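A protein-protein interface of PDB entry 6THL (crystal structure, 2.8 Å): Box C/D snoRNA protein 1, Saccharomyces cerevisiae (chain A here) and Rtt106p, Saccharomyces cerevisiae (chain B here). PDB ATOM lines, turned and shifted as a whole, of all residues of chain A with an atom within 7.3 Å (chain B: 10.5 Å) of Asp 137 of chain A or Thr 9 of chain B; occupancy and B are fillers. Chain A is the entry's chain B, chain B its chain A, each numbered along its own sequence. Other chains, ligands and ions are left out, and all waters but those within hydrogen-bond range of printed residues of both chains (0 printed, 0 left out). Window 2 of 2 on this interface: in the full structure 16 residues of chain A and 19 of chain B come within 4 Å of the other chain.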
ATOM      1  N   LEU A  18      22.255   9.454  -2.357  1.00  0.00           N
ATOM      2  CA  LEU A  18      22.251   9.747  -0.920  1.00  0.00           C
ATOM      3  C   LEU A  18      23.644   9.529  -0.353  1.00  0.00           C
ATOM      4  O   LEU A  18      24.288   8.500  -0.579  1.00  0.00           O
ATOM      5  CB  LEU A  18      21.229   8.911  -0.152  1.00  0.00           C
ATOM      6  CG  LEU A  18      19.811   9.083  -0.657  1.00  0.00           C
ATOM      7  CD1 LEU A  18      18.836   8.228   0.137  1.00  0.00           C
ATOM      8  CD2 LEU A  18      19.460  10.546  -0.578  1.00  0.00           C
ATOM      9  N   LEU A  20      26.168   9.474   2.846  1.00  0.00           N
ATOM     10  CA  LEU A  20      26.234   9.177   4.244  1.00  0.00           C
ATOM     11  C   LEU A  20      27.292  10.084   4.860  1.00  0.00           C
ATOM     12  O   LEU A  20      28.172  10.598   4.142  1.00  0.00           O
ATOM     13  CB  LEU A  20      26.578   7.698   4.361  1.00  0.00           C
ATOM     14  CG  LEU A  20      25.482   6.764   3.790  1.00  0.00           C
ATOM     15  CD1 LEU A  20      25.897   5.294   3.839  1.00  0.00           C
ATOM     16  CD2 LEU A  20      24.127   6.952   4.501  1.00  0.00           C
ATOM     17  N   PRO A  21      27.242  10.295   6.183  1.00  0.00           N
ATOM     18  CA  PRO A  21      28.420  10.898   6.842  1.00  0.00           C
ATOM     19  C   PRO A  21      29.668  10.082   6.553  1.00  0.00           C
ATOM     20  O   PRO A  21      29.628   8.856   6.470  1.00  0.00           O
ATOM     21  CB  PRO A  21      28.106  10.848   8.326  1.00  0.00           C
ATOM     22  CG  PRO A  21      26.771  10.220   8.473  1.00  0.00           C
ATOM     23  CD  PRO A  21      26.314   9.685   7.142  1.00  0.00           C
ATOM     24  N   MET A  24      31.246   6.783   7.781  1.00  0.00           N
ATOM     25  CA  MET A  24      30.582   5.514   7.570  1.00  0.00           C
ATOM     26  C   MET A  24      31.412   4.702   6.606  1.00  0.00           C
ATOM     27  O   MET A  24      31.975   5.244   5.675  1.00  0.00           O
ATOM     28  CB  MET A  24      29.157   5.704   7.051  1.00  0.00           C
ATOM     29  CG  MET A  24      28.218   6.408   8.016  1.00  0.00           C
ATOM     30  SD  MET A  24      27.844   5.437   9.486  1.00  0.00           S
ATOM     31  CE  MET A  24      27.476   6.798  10.579  1.00  0.00           C
ATOM     32  N   ARG A  26      30.691   2.734   4.271  1.00  0.00           N
ATOM     33  CA  ARG A  26      30.236   2.818   2.890  1.00  0.00           C
ATOM     34  C   ARG A  26      30.769   4.085   2.261  1.00  0.00           C
ATOM     35  O   ARG A  26      31.175   4.092   1.087  1.00  0.00           O
ATOM     36  CB  ARG A  26      28.709   2.783   2.750  1.00  0.00           C
ATOM     37  CG  ARG A  26      28.223   2.851   1.297  1.00  0.00           C
ATOM     38  CD  ARG A  26      26.796   2.329   1.062  1.00  0.00           C
ATOM     39  NE  ARG A  26      26.550   2.221  -0.376  1.00  0.00           N
ATOM     40  CZ  ARG A  26      26.547   1.098  -1.090  1.00  0.00           C
ATOM     41  NH1 ARG A  26      26.656  -0.076  -0.506  1.00  0.00           N
ATOM     42  NH2 ARG A  26      26.359   1.160  -2.416  1.00  0.00           N
ATOM     43  N   LYS A 126      18.272  -1.947  -6.091  1.00  0.00           N
ATOM     44  CA  LYS A 126      17.262  -1.756  -5.081  1.00  0.00           C
ATOM     45  C   LYS A 126      16.609  -0.414  -5.317  1.00  0.00           C
ATOM     46  O   LYS A 126      17.173   0.427  -6.028  1.00  0.00           O
ATOM     47  CB  LYS A 126      17.885  -1.925  -3.691  1.00  0.00           C
ATOM     48  CG  LYS A 126      18.572  -0.710  -3.128  1.00  0.00           C
ATOM     49  CD  LYS A 126      19.781  -1.100  -2.283  1.00  0.00           C
ATOM     50  CE  LYS A 126      19.412  -1.790  -0.998  1.00  0.00           C
ATOM     51  NZ  LYS A 126      20.593  -1.966  -0.094  1.00  0.00           N
ATOM     52  N   THR A 127      15.413  -0.208  -4.762  1.00  0.00           N
ATOM     53  CA  THR A 127      14.555   0.927  -5.192  1.00  0.00           C
ATOM     54  C   THR A 127      14.079   1.729  -4.012  1.00  0.00           C
ATOM     55  O   THR A 127      13.905   1.196  -2.939  1.00  0.00           O
ATOM     56  CB  THR A 127      13.352   0.435  -6.043  1.00  0.00           C
ATOM     57  OG1 THR A 127      13.001   1.421  -7.004  1.00  0.00           O
ATOM     58  CG2 THR A 127      12.099   0.048  -5.193  1.00  0.00           C
ATOM     59  N   PHE A 128      13.878   3.021  -4.227  1.00  0.00           N
ATOM     60  CA  PHE A 128      13.643   3.965  -3.140  1.00  0.00           C
ATOM     61  C   PHE A 128      12.482   4.887  -3.498  1.00  0.00           C
ATOM     62  O   PHE A 128      12.301   5.178  -4.685  1.00  0.00           O
ATOM     63  CB  PHE A 128      14.878   4.859  -2.913  1.00  0.00           C
ATOM     64  CG  PHE A 128      16.109   4.125  -2.482  1.00  0.00           C
ATOM     65  CD1 PHE A 128      16.408   3.975  -1.131  1.00  0.00           C
ATOM     66  CD2 PHE A 128      16.997   3.614  -3.431  1.00  0.00           C
ATOM     67  CE1 PHE A 128      17.550   3.297  -0.730  1.00  0.00           C
ATOM     68  CE2 PHE A 128      18.150   2.936  -3.037  1.00  0.00           C
ATOM     69  CZ  PHE A 128      18.425   2.774  -1.684  1.00  0.00           C
ATOM     70  N   PRO A 129      11.733   5.378  -2.478  1.00  0.00           N
ATOM     71  CA  PRO A 129      10.725   6.425  -2.674  1.00  0.00           C
ATOM     72  C   PRO A 129      11.246   7.673  -3.424  1.00  0.00           C
ATOM     73  O   PRO A 129      10.695   8.078  -4.471  1.00  0.00           O
ATOM     74  CB  PRO A 129      10.316   6.783  -1.236  1.00  0.00           C
ATOM     75  CG  PRO A 129      10.571   5.546  -0.428  1.00  0.00           C
ATOM     76  CD  PRO A 129      11.748   4.875  -1.081  1.00  0.00           C
ATOM     77  N   ILE A 135      17.510   9.711   5.436  1.00  0.00           N
ATOM     78  CA  ILE A 135      18.208   8.664   4.664  1.00  0.00           C
ATOM     79  C   ILE A 135      17.923   7.241   5.136  1.00  0.00           C
ATOM     80  O   ILE A 135      18.030   6.952   6.330  1.00  0.00           O
ATOM     81  CB  ILE A 135      19.746   8.867   4.689  1.00  0.00           C
ATOM     82  CG1 ILE A 135      20.132  10.045   3.789  1.00  0.00           C
ATOM     83  CG2 ILE A 135      20.474   7.609   4.223  1.00  0.00           C
ATOM     84  CD1 ILE A 135      21.617  10.290   3.640  1.00  0.00           C
ATOM     85  N   MET A 136      17.631   6.335   4.198  1.00  0.00           N
ATOM     86  CA  MET A 136      17.155   5.011   4.597  1.00  0.00           C
ATOM     87  C   MET A 136      17.369   3.903   3.587  1.00  0.00           C
ATOM     88  O   MET A 136      16.889   3.994   2.465  1.00  0.00           O
ATOM     89  CB  MET A 136      15.661   5.112   4.935  1.00  0.00           C
ATOM     90  CG  MET A 136      15.060   3.865   5.564  1.00  0.00           C
ATOM     91  SD  MET A 136      13.797   4.225   6.812  1.00  0.00           S
ATOM     92  CE  MET A 136      12.417   4.922   5.881  1.00  0.00           C
ATOM     93  N   ASP A 137      18.061   2.843   4.022  1.00  0.00           N
ATOM     94  CA  ASP A 137      18.268   1.570   3.268  1.00  0.00           C
ATOM     95  C   ASP A 137      16.926   0.976   2.754  1.00  0.00           C
ATOM     96  O   ASP A 137      15.874   1.379   3.204  1.00  0.00           O
ATOM     97  CB  ASP A 137      18.956   0.607   4.250  1.00  0.00           C
ATOM     98  CG  ASP A 137      19.599  -0.642   3.606  1.00  0.00           C
ATOM     99  OD1 ASP A 137      19.490  -0.918   2.396  1.00  0.00           O
ATOM    100  OD2 ASP A 137      20.238  -1.380   4.390  1.00  0.00           O
ATOM    101  N   SER A 138      16.959   0.040   1.815  1.00  0.00           N
ATOM    102  CA  SER A 138      15.751  -0.592   1.291  1.00  0.00           C
ATOM    103  C   SER A 138      15.908  -2.103   1.010  1.00  0.00           C
ATOM    104  O   SER A 138      17.009  -2.624   0.809  1.00  0.00           O
ATOM    105  CB  SER A 138      15.299   0.118   0.010  1.00  0.00           C
ATOM    106  OG  SER A 138      14.254  -0.596  -0.655  1.00  0.00           O
ATOM    107  N   LYS A 139      14.790  -2.813   1.028  1.00  0.00           N
ATOM    108  CA  LYS A 139      14.788  -4.225   0.696  1.00  0.00           C
ATOM    109  C   LYS A 139      13.769  -4.486  -0.411  1.00  0.00           C
ATOM    110  O   LYS A 139      13.369  -5.629  -0.652  1.00  0.00           O
ATOM    111  CB  LYS A 139      14.513  -5.037   1.952  1.00  0.00           C
ATOM    112  CG  LYS A 139      15.500  -4.691   3.048  1.00  0.00           C
ATOM    113  CD  LYS A 139      15.622  -5.732   4.125  1.00  0.00           C
ATOM    114  CE  LYS A 139      16.292  -5.109   5.337  1.00  0.00           C
ATOM    115  NZ  LYS A 139      16.544  -6.096   6.426  1.00  0.00           N
ATOM    116  N   LYS A 140      13.386  -3.407  -1.094  1.00  0.00           N
ATOM    117  CA  LYS A 140      12.503  -3.461  -2.227  1.00  0.00           C
ATOM    118  C   LYS A 140      13.409  -3.433  -3.417  1.00  0.00           C
ATOM    119  O   LYS A 140      14.144  -2.468  -3.604  1.00  0.00           O
ATOM    120  CB  LYS A 140      11.590  -2.214  -2.292  1.00  0.00           C
ATOM    121  CG  LYS A 140      10.640  -1.984  -1.119  1.00  0.00           C
ATOM    122  CD  LYS A 140       9.749  -3.167  -0.853  1.00  0.00           C
ATOM    123  CE  LYS A 140       8.892  -2.876   0.351  1.00  0.00           C
ATOM    124  NZ  LYS A 140       8.635  -4.132   1.103  1.00  0.00           N
ATOM    125  N   ILE A 161      22.138   4.608  -2.620  1.00  0.00           N
ATOM    126  CA  ILE A 161      22.825   4.992  -1.406  1.00  0.00           C
ATOM    127  C   ILE A 161      24.300   4.994  -1.767  1.00  0.00           C
ATOM    128  O   ILE A 161      24.960   3.938  -1.916  1.00  0.00           O
ATOM    129  CB  ILE A 161      22.512   4.073  -0.240  1.00  0.00           C
ATOM    130  CG1 ILE A 161      21.120   4.430   0.261  1.00  0.00           C
ATOM    131  CG2 ILE A 161      23.518   4.319   0.878  1.00  0.00           C
ATOM    132  CD1 ILE A 161      20.487   3.377   1.110  1.00  0.00           C
ATOM    133  N   THR A 165      23.991  -0.689  -5.616  1.00  0.00           N
ATOM    134  CA  THR A 165      24.239  -2.044  -5.182  1.00  0.00           C
ATOM    135  C   THR A 165      23.478  -2.915  -6.208  1.00  0.00           C
ATOM    136  O   THR A 165      22.420  -2.500  -6.690  1.00  0.00           O
ATOM    137  CB  THR A 165      23.708  -2.221  -3.749  1.00  0.00           C
ATOM    138  OG1 THR A 165      24.315  -1.232  -2.890  1.00  0.00           O
ATOM    139  CG2 THR A 165      23.959  -3.613  -3.235  1.00  0.00           C
ATOM    140  N   TYR A 179      14.424  -9.276   1.499  1.00  0.00           N
ATOM    141  CA  TYR A 179      14.367  -8.635   0.177  1.00  0.00           C
ATOM    142  C   TYR A 179      13.168  -9.132  -0.619  1.00  0.00           C
ATOM    143  O   TYR A 179      12.919 -10.331  -0.700  1.00  0.00           O
ATOM    144  CB  TYR A 179      15.688  -8.835  -0.609  1.00  0.00           C
ATOM    145  CG  TYR A 179      16.780  -8.019   0.022  1.00  0.00           C
ATOM    146  CD1 TYR A 179      17.362  -8.452   1.197  1.00  0.00           C
ATOM    147  CD2 TYR A 179      17.160  -6.769  -0.491  1.00  0.00           C
ATOM    148  CE1 TYR A 179      18.311  -7.700   1.836  1.00  0.00           C
ATOM    149  CE2 TYR A 179      18.109  -6.005   0.158  1.00  0.00           C
ATOM    150  CZ  TYR A 179      18.672  -6.498   1.328  1.00  0.00           C
ATOM    151  OH  TYR A 179      19.621  -5.857   2.049  1.00  0.00           O
ATOM    152  N   GLU B   5      17.462  -1.703  12.089  1.00  0.00           N
ATOM    153  CA  GLU B   5      18.293  -1.127  13.183  1.00  0.00           C
ATOM    154  C   GLU B   5      19.730  -0.866  12.699  1.00  0.00           C
ATOM    155  O   GLU B   5      20.178   0.261  12.759  1.00  0.00           O
ATOM    156  CB  GLU B   5      18.299  -2.014  14.444  1.00  0.00           C
ATOM    157  CG  GLU B   5      17.177  -1.762  15.443  1.00  0.00           C
ATOM    158  CD  GLU B   5      17.496  -0.700  16.495  1.00  0.00           C
ATOM    159  OE1 GLU B   5      18.291  -0.942  17.459  1.00  0.00           O
ATOM    160  OE2 GLU B   5      16.922   0.401  16.358  1.00  0.00           O
ATOM    161  N   ILE B   6      20.467  -1.881  12.247  1.00  0.00           N
ATOM    162  CA  ILE B   6      21.802  -1.609  11.684  1.00  0.00           C
ATOM    163  C   ILE B   6      21.948  -2.007  10.239  1.00  0.00           C
ATOM    164  O   ILE B   6      21.537  -3.055   9.835  1.00  0.00           O
ATOM    165  CB  ILE B   6      22.984  -2.050  12.600  1.00  0.00           C
ATOM    166  CG1 ILE B   6      23.362  -3.493  12.484  1.00  0.00           C
ATOM    167  CG2 ILE B   6      22.622  -1.762  14.047  1.00  0.00           C
ATOM    168  CD1 ILE B   6      23.889  -4.056  13.805  1.00  0.00           C
ATOM    169  N   SER B   7      22.464  -1.091   9.444  1.00  0.00           N
ATOM    170  CA  SER B   7      22.643  -1.333   8.032  1.00  0.00           C
ATOM    171  C   SER B   7      23.742  -0.396   7.507  1.00  0.00           C
ATOM    172  O   SER B   7      24.348   0.360   8.296  1.00  0.00           O
ATOM    173  CB  SER B   7      21.353  -1.055   7.314  1.00  0.00           C
ATOM    174  OG  SER B   7      21.291   0.333   7.060  1.00  0.00           O
ATOM    175  N   GLU B   8      23.949  -0.414   6.187  1.00  0.00           N
ATOM    176  CA  GLU B   8      24.965   0.396   5.547  1.00  0.00           C
ATOM    177  C   GLU B   8      24.911   1.872   5.772  1.00  0.00           C
ATOM    178  O   GLU B   8      25.841   2.537   5.344  1.00  0.00           O
ATOM    179  CB  GLU B   8      25.008   0.182   4.048  1.00  0.00           C
ATOM    180  CG  GLU B   8      23.981   0.939   3.238  1.00  0.00           C
ATOM    181  CD  GLU B   8      23.799   0.328   1.843  1.00  0.00           C
ATOM    182  OE1 GLU B   8      24.154   1.006   0.816  1.00  0.00           O
ATOM    183  OE2 GLU B   8      23.336  -0.851   1.795  1.00  0.00           O
ATOM    184  N   THR B   9      23.876   2.406   6.427  1.00  0.00           N
ATOM    185  CA  THR B   9      23.727   3.879   6.534  1.00  0.00           C
ATOM    186  C   THR B   9      24.123   4.450   7.898  1.00  0.00           C
ATOM    187  O   THR B   9      24.248   5.665   8.057  1.00  0.00           O
ATOM    188  CB  THR B   9      22.270   4.289   6.280  1.00  0.00           C
ATOM    189  OG1 THR B   9      21.491   3.862   7.401  1.00  0.00           O
ATOM    190  CG2 THR B   9      21.719   3.638   4.985  1.00  0.00           C
ATOM    191  N   ASN B  10      24.247   3.580   8.894  1.00  0.00           N
ATOM    192  CA  ASN B  10      24.742   3.970  10.230  1.00  0.00           C
ATOM    193  C   ASN B  10      25.923   3.105  10.720  1.00  0.00           C
ATOM    194  O   ASN B  10      26.286   3.173  11.893  1.00  0.00           O
ATOM    195  CB  ASN B  10      23.600   3.866  11.254  1.00  0.00           C
ATOM    196  CG  ASN B  10      23.060   2.461  11.384  1.00  0.00           C
ATOM    197  OD1 ASN B  10      23.131   1.640  10.445  1.00  0.00           O
ATOM    198  ND2 ASN B  10      22.530   2.165  12.547  1.00  0.00           N
ATOM    199  N   THR B  11      26.461   2.272   9.824  1.00  0.00           N
ATOM    200  CA  THR B  11      27.552   1.351  10.127  1.00  0.00           C
ATOM    201  C   THR B  11      28.883   2.064   9.936  1.00  0.00           C
ATOM    202  O   THR B  11      29.256   2.440   8.817  1.00  0.00           O
ATOM    203  CB  THR B  11      27.553   0.110   9.210  1.00  0.00           C
ATOM    204  OG1 THR B  11      26.478  -0.787   9.561  1.00  0.00           O
ATOM    205  CG2 THR B  11      28.838  -0.603   9.349  1.00  0.00           C
ATOM    206  N   ILE B  12      29.597   2.233  11.038  1.00  0.00           N
ATOM    207  CA  ILE B  12      30.916   2.841  10.996  1.00  0.00           C
ATOM    208  C   ILE B  12      31.899   1.872  10.392  1.00  0.00           C
ATOM    209  O   ILE B  12      32.665   2.252   9.541  1.00  0.00           O
ATOM    210  CB  ILE B  12      31.419   3.275  12.401  1.00  0.00           C
ATOM    211  CG1 ILE B  12      30.465   4.307  13.001  1.00  0.00           C
ATOM    212  CG2 ILE B  12      32.826   3.869  12.333  1.00  0.00           C
ATOM    213  CD1 ILE B  12      30.101   5.393  12.029  1.00  0.00           C
ATOM    214  N   PHE B  13      31.856   0.628  10.849  1.00  0.00           N
ATOM    215  CA  PHE B  13      32.853  -0.377  10.512  1.00  0.00           C
ATOM    216  C   PHE B  13      32.115  -1.696  10.570  1.00  0.00           C
ATOM    217  O   PHE B  13      31.164  -1.832  11.333  1.00  0.00           O
ATOM    218  CB  PHE B  13      34.047  -0.313  11.511  1.00  0.00           C
ATOM    219  CG  PHE B  13      35.028  -1.450  11.387  1.00  0.00           C
ATOM    220  CD1 PHE B  13      35.110  -2.419  12.346  1.00  0.00           C
ATOM    221  CD2 PHE B  13      35.860  -1.552  10.291  1.00  0.00           C
ATOM    222  CE1 PHE B  13      36.014  -3.467  12.212  1.00  0.00           C
ATOM    223  CE2 PHE B  13      36.775  -2.596  10.152  1.00  0.00           C
ATOM    224  CZ  PHE B  13      36.852  -3.554  11.115  1.00  0.00           C
ATOM    225  N   LYS B  14      32.546  -2.641   9.751  1.00  0.00           N
ATOM    226  CA  LYS B  14      31.888  -3.920   9.626  1.00  0.00           C
ATOM    227  C   LYS B  14      32.922  -4.844   9.020  1.00  0.00           C
ATOM    228  O   LYS B  14      33.331  -4.630   7.875  1.00  0.00           O
ATOM    229  CB  LYS B  14      30.674  -3.789   8.677  1.00  0.00           C
ATOM    230  CG  LYS B  14      29.736  -5.008   8.579  1.00  0.00           C
ATOM    231  CD  LYS B  14      28.531  -4.744   7.660  1.00  0.00           C
ATOM    232  CE  LYS B  14      27.381  -3.932   8.320  1.00  0.00           C
ATOM    233  NZ  LYS B  14      26.570  -3.027   7.414  1.00  0.00           N
ATOM    234  N   VAL B  31      31.016  -5.211  14.436  1.00  0.00           N
ATOM    235  CA  VAL B  31      30.355  -4.012  13.911  1.00  0.00           C
ATOM    236  C   VAL B  31      30.349  -2.844  14.862  1.00  0.00           C
ATOM    237  O   VAL B  31      29.917  -2.971  16.032  1.00  0.00           O
ATOM    238  CB  VAL B  31      28.872  -4.257  13.551  1.00  0.00           C
ATOM    239  CG1 VAL B  31      28.234  -2.972  13.058  1.00  0.00           C
ATOM    240  CG2 VAL B  31      28.735  -5.313  12.478  1.00  0.00           C
ATOM    241  N   PHE B  32      30.820  -1.703  14.351  1.00  0.00           N
ATOM    242  CA  PHE B  32      30.632  -0.416  15.033  1.00  0.00           C
ATOM    243  C   PHE B  32      29.533   0.367  14.315  1.00  0.00           C
ATOM    244  O   PHE B  32      29.517   0.501  13.086  1.00  0.00           O
ATOM    245  CB  PHE B  32      31.917   0.430  15.041  1.00  0.00           C
ATOM    246  CG  PHE B  32      33.173  -0.300  15.460  1.00  0.00           C
ATOM    247  CD1 PHE B  32      34.424   0.261  15.170  1.00  0.00           C
ATOM    248  CD2 PHE B  32      33.139  -1.502  16.145  1.00  0.00           C
ATOM    249  CE1 PHE B  32      35.597  -0.379  15.550  1.00  0.00           C
ATOM    250  CE2 PHE B  32      34.323  -2.155  16.511  1.00  0.00           C
ATOM    251  CZ  PHE B  32      35.553  -1.590  16.225  1.00  0.00           C
ATOM    252  N   TYR B  33      28.590   0.880  15.051  1.00  0.00           N
ATOM    253  CA  TYR B  33      27.549   1.657  14.372  1.00  0.00           C
ATOM    254  C   TYR B  33      26.908   2.619  15.302  1.00  0.00           C
ATOM    255  O   TYR B  33      26.977   2.433  16.514  1.00  0.00           O
ATOM    256  CB  TYR B  33      26.500   0.716  13.859  1.00  0.00           C
ATOM    257  CG  TYR B  33      25.699   0.070  14.973  1.00  0.00           C
ATOM    258  CD1 TYR B  33      24.523   0.671  15.423  1.00  0.00           C
ATOM    259  CD2 TYR B  33      26.102  -1.142  15.577  1.00  0.00           C
ATOM    260  CE1 TYR B  33      23.761   0.094  16.435  1.00  0.00           C
ATOM    261  CE2 TYR B  33      25.334  -1.727  16.598  1.00  0.00           C
ATOM    262  CZ  TYR B  33      24.164  -1.089  17.019  1.00  0.00           C
ATOM    263  OH  TYR B  33      23.359  -1.561  18.005  1.00  0.00           O
ATOM    264  N   LEU B  34      26.291   3.652  14.753  1.00  0.00           N
ATOM    265  CA  LEU B  34      25.507   4.622  15.576  1.00  0.00           C
ATOM    266  C   LEU B  34      24.045   4.211  15.635  1.00  0.00           C
ATOM    267  O   LEU B  34      23.388   4.070  14.608  1.00  0.00           O
ATOM    268  CB  LEU B  34      25.616   6.043  15.026  1.00  0.00           C
ATOM    269  CG  LEU B  34      27.030   6.425  14.593  1.00  0.00           C
ATOM    270  CD1 LEU B  34      27.071   7.883  14.186  1.00  0.00           C
ATOM    271  CD2 LEU B  34      28.033   6.132  15.697  1.00  0.00           C
ATOM    272  N   SER B  35      23.573   3.966  16.842  1.00  0.00           N
ATOM    273  CA  SER B  35      22.160   3.670  17.120  1.00  0.00           C
ATOM    274  C   SER B  35      21.234   4.671  16.418  1.00  0.00           C
ATOM    275  O   SER B  35      21.504   5.886  16.427  1.00  0.00           O
ATOM    276  CB  SER B  35      21.926   3.715  18.643  1.00  0.00           C
ATOM    277  OG  SER B  35      20.572   3.960  18.988  1.00  0.00           O
ATOM    278  N   ASN B  36      20.160   4.170  15.800  1.00  0.00           N
ATOM    279  CA  ASN B  36      19.161   5.064  15.197  1.00  0.00           C
ATOM    280  C   ASN B  36      18.227   5.645  16.227  1.00  0.00           C
ATOM    281  O   ASN B  36      17.757   6.746  16.032  1.00  0.00           O
ATOM    282  CB  ASN B  36      18.412   4.413  14.058  1.00  0.00           C
ATOM    283  CG  ASN B  36      19.217   4.429  12.782  1.00  0.00           C
ATOM    284  OD1 ASN B  36      19.994   5.359  12.530  1.00  0.00           O
ATOM    285  ND2 ASN B  36      19.059   3.394  11.972  1.00  0.00           N
ATOM    286  N   GLY B  39      21.462   8.362  18.114  1.00  0.00           N
ATOM    287  CA  GLY B  39      22.776   8.748  17.523  1.00  0.00           C
ATOM    288  C   GLY B  39      24.076   8.304  18.222  1.00  0.00           C
ATOM    289  O   GLY B  39      25.146   8.805  17.900  1.00  0.00           O
ATOM    290  N   ASN B  49      21.969 -11.362  11.776  1.00  0.00           N
ATOM    291  CA  ASN B  49      21.427 -10.192  12.487  1.00  0.00           C
ATOM    292  C   ASN B  49      21.079 -10.478  13.967  1.00  0.00           C
ATOM    293  O   ASN B  49      20.435  -9.653  14.605  1.00  0.00           O
ATOM    294  CB  ASN B  49      20.185  -9.637  11.754  1.00  0.00           C
ATOM    295  CG  ASN B  49      20.480  -9.201  10.316  1.00  0.00           C
ATOM    296  OD1 ASN B  49      20.086  -9.874   9.352  1.00  0.00           O
ATOM    297  ND2 ASN B  49      21.178  -8.072  10.166  1.00  0.00           N
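OD2 of Asp 137 of chain A sits close to OG of Ser 7 of chain B.
The guanidinium group (NE) of Arg 26 of chain A is in salt-bridge range of the side-chain carboxylate (OE1) of Glu 8 of chain B, 2.9 Å away.
The side-chain amino group (NZ) of Lys 126 of chain A lies within salt-bridge range of the side-chain carboxylate (OE2) of Glu 8 of chain B.
N of Thr 11 of chain B sits at hydrogen-bond distance from SD of Met 24 of chain A.
SD of Met 24 of chain A lies close to O of Asn 10 of chain B (3.7 Å).
The side-chain hydroxyl of Ser 7 of chain B sits close to the backbone NH of Thr 9 of chain B (3.4 Å).
O of Ser 7 of chain B lies close to OD1 of Asn 10 of chain B, at 2.8 Å.
O of Asn 10 of chain B lies within hydrogen-bond range of N of Leu 34 of chain B.
OG1 of Thr 11 of chain B lies within hydrogen-bond range of NZ of Lys 14 of chain B, at 3.1 Å.
The guanidinium group (NE) of Arg 26 of chain A sits at hydrogen-bond distance from the backbone carbonyl oxygen (O) of Ile 161 of chain A (2.8 Å).
The side-chain carboxylate of Asp 137 of chain A is in salt-bridge range of the side-chain amino group of Lys 126 of chain A, 2.9 Å away.
Among the printed residues, pairs that only touch across the chains: Leu 20 of chain A with Glu 8 of chain B, Leu 20 of chain A with Thr 9 of chain B, Met 24 of chain A with Thr 9 of chain B, Met 24 of chain A with Ile 12 of chain B, Met 24 of chain A with Leu 34 of chain B, Asp 137 of chain A with Glu 8 of chain B, Asp 137 of chain A with Thr 9 of chain B and Ile 161 of chain A with Glu 8 of chain B.
Thr 9 of chain B touches just these residues of chain A: Leu 20 (3.7 Å), Met 24 (3.9 Å) and Asp 137 (3.9 Å).
No residue of chain B comes within 4 Å of Ser 138 of chain A.
Of the printed residues of chain B, Arg 26 of chain A touches Glu 8.
Of the printed residues of chain B, Met 24 of chain A touches Thr 9 (3.9 Å), Asn 10 (3.3 Å), Thr 11 (3.4 Å), Ile 12 (3.3 Å) and Leu 34 (3.8 Å).
Of the printed residues of chain B, Leu 20 of chain A touches Glu 8 and Thr 9.
Of the printed residues of chain A, Thr 11 of chain B touches Met 24.
Printed residues of chain B within 4 Å of Ile 161 of chain A: Glu 8 (3.4 Å).
Tyr 33 of chain B touches none of the printed residues of chain A.
Val 31 of chain B touches none of the printed residues of chain A.
The nearest residue of chain A that does not touch Thr 9 of chain B is Ile 161 of chain A (4.1 Å).
Of the 18 printed residues of chain B, 7 touch a printed residue of chain A.
Hydrophobic or aromatic side chains of chain B that line the printed part of chain A: Ile 12 and Leu 34.
Of the 18 printed residues of chain A, 6 touch a printed residue of chain B.
Printed residues of chain A that touch a printed residue of chain B: Leu 20, Met 24, Arg 26, Lys 126, Asp 137 and Ile 161.
Among the printed residues, 13 pairs touch across the chains.
Among the printed residues, Asp or Glu carboxylates within 4 Å of a Lys or Arg side-chain nitrogen of the other chain: Arg 26 of chain A with Glu 8 of chain B (2.9 Å) and Lys 126 of chain A with Glu 8 of chain B (3.5 Å).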
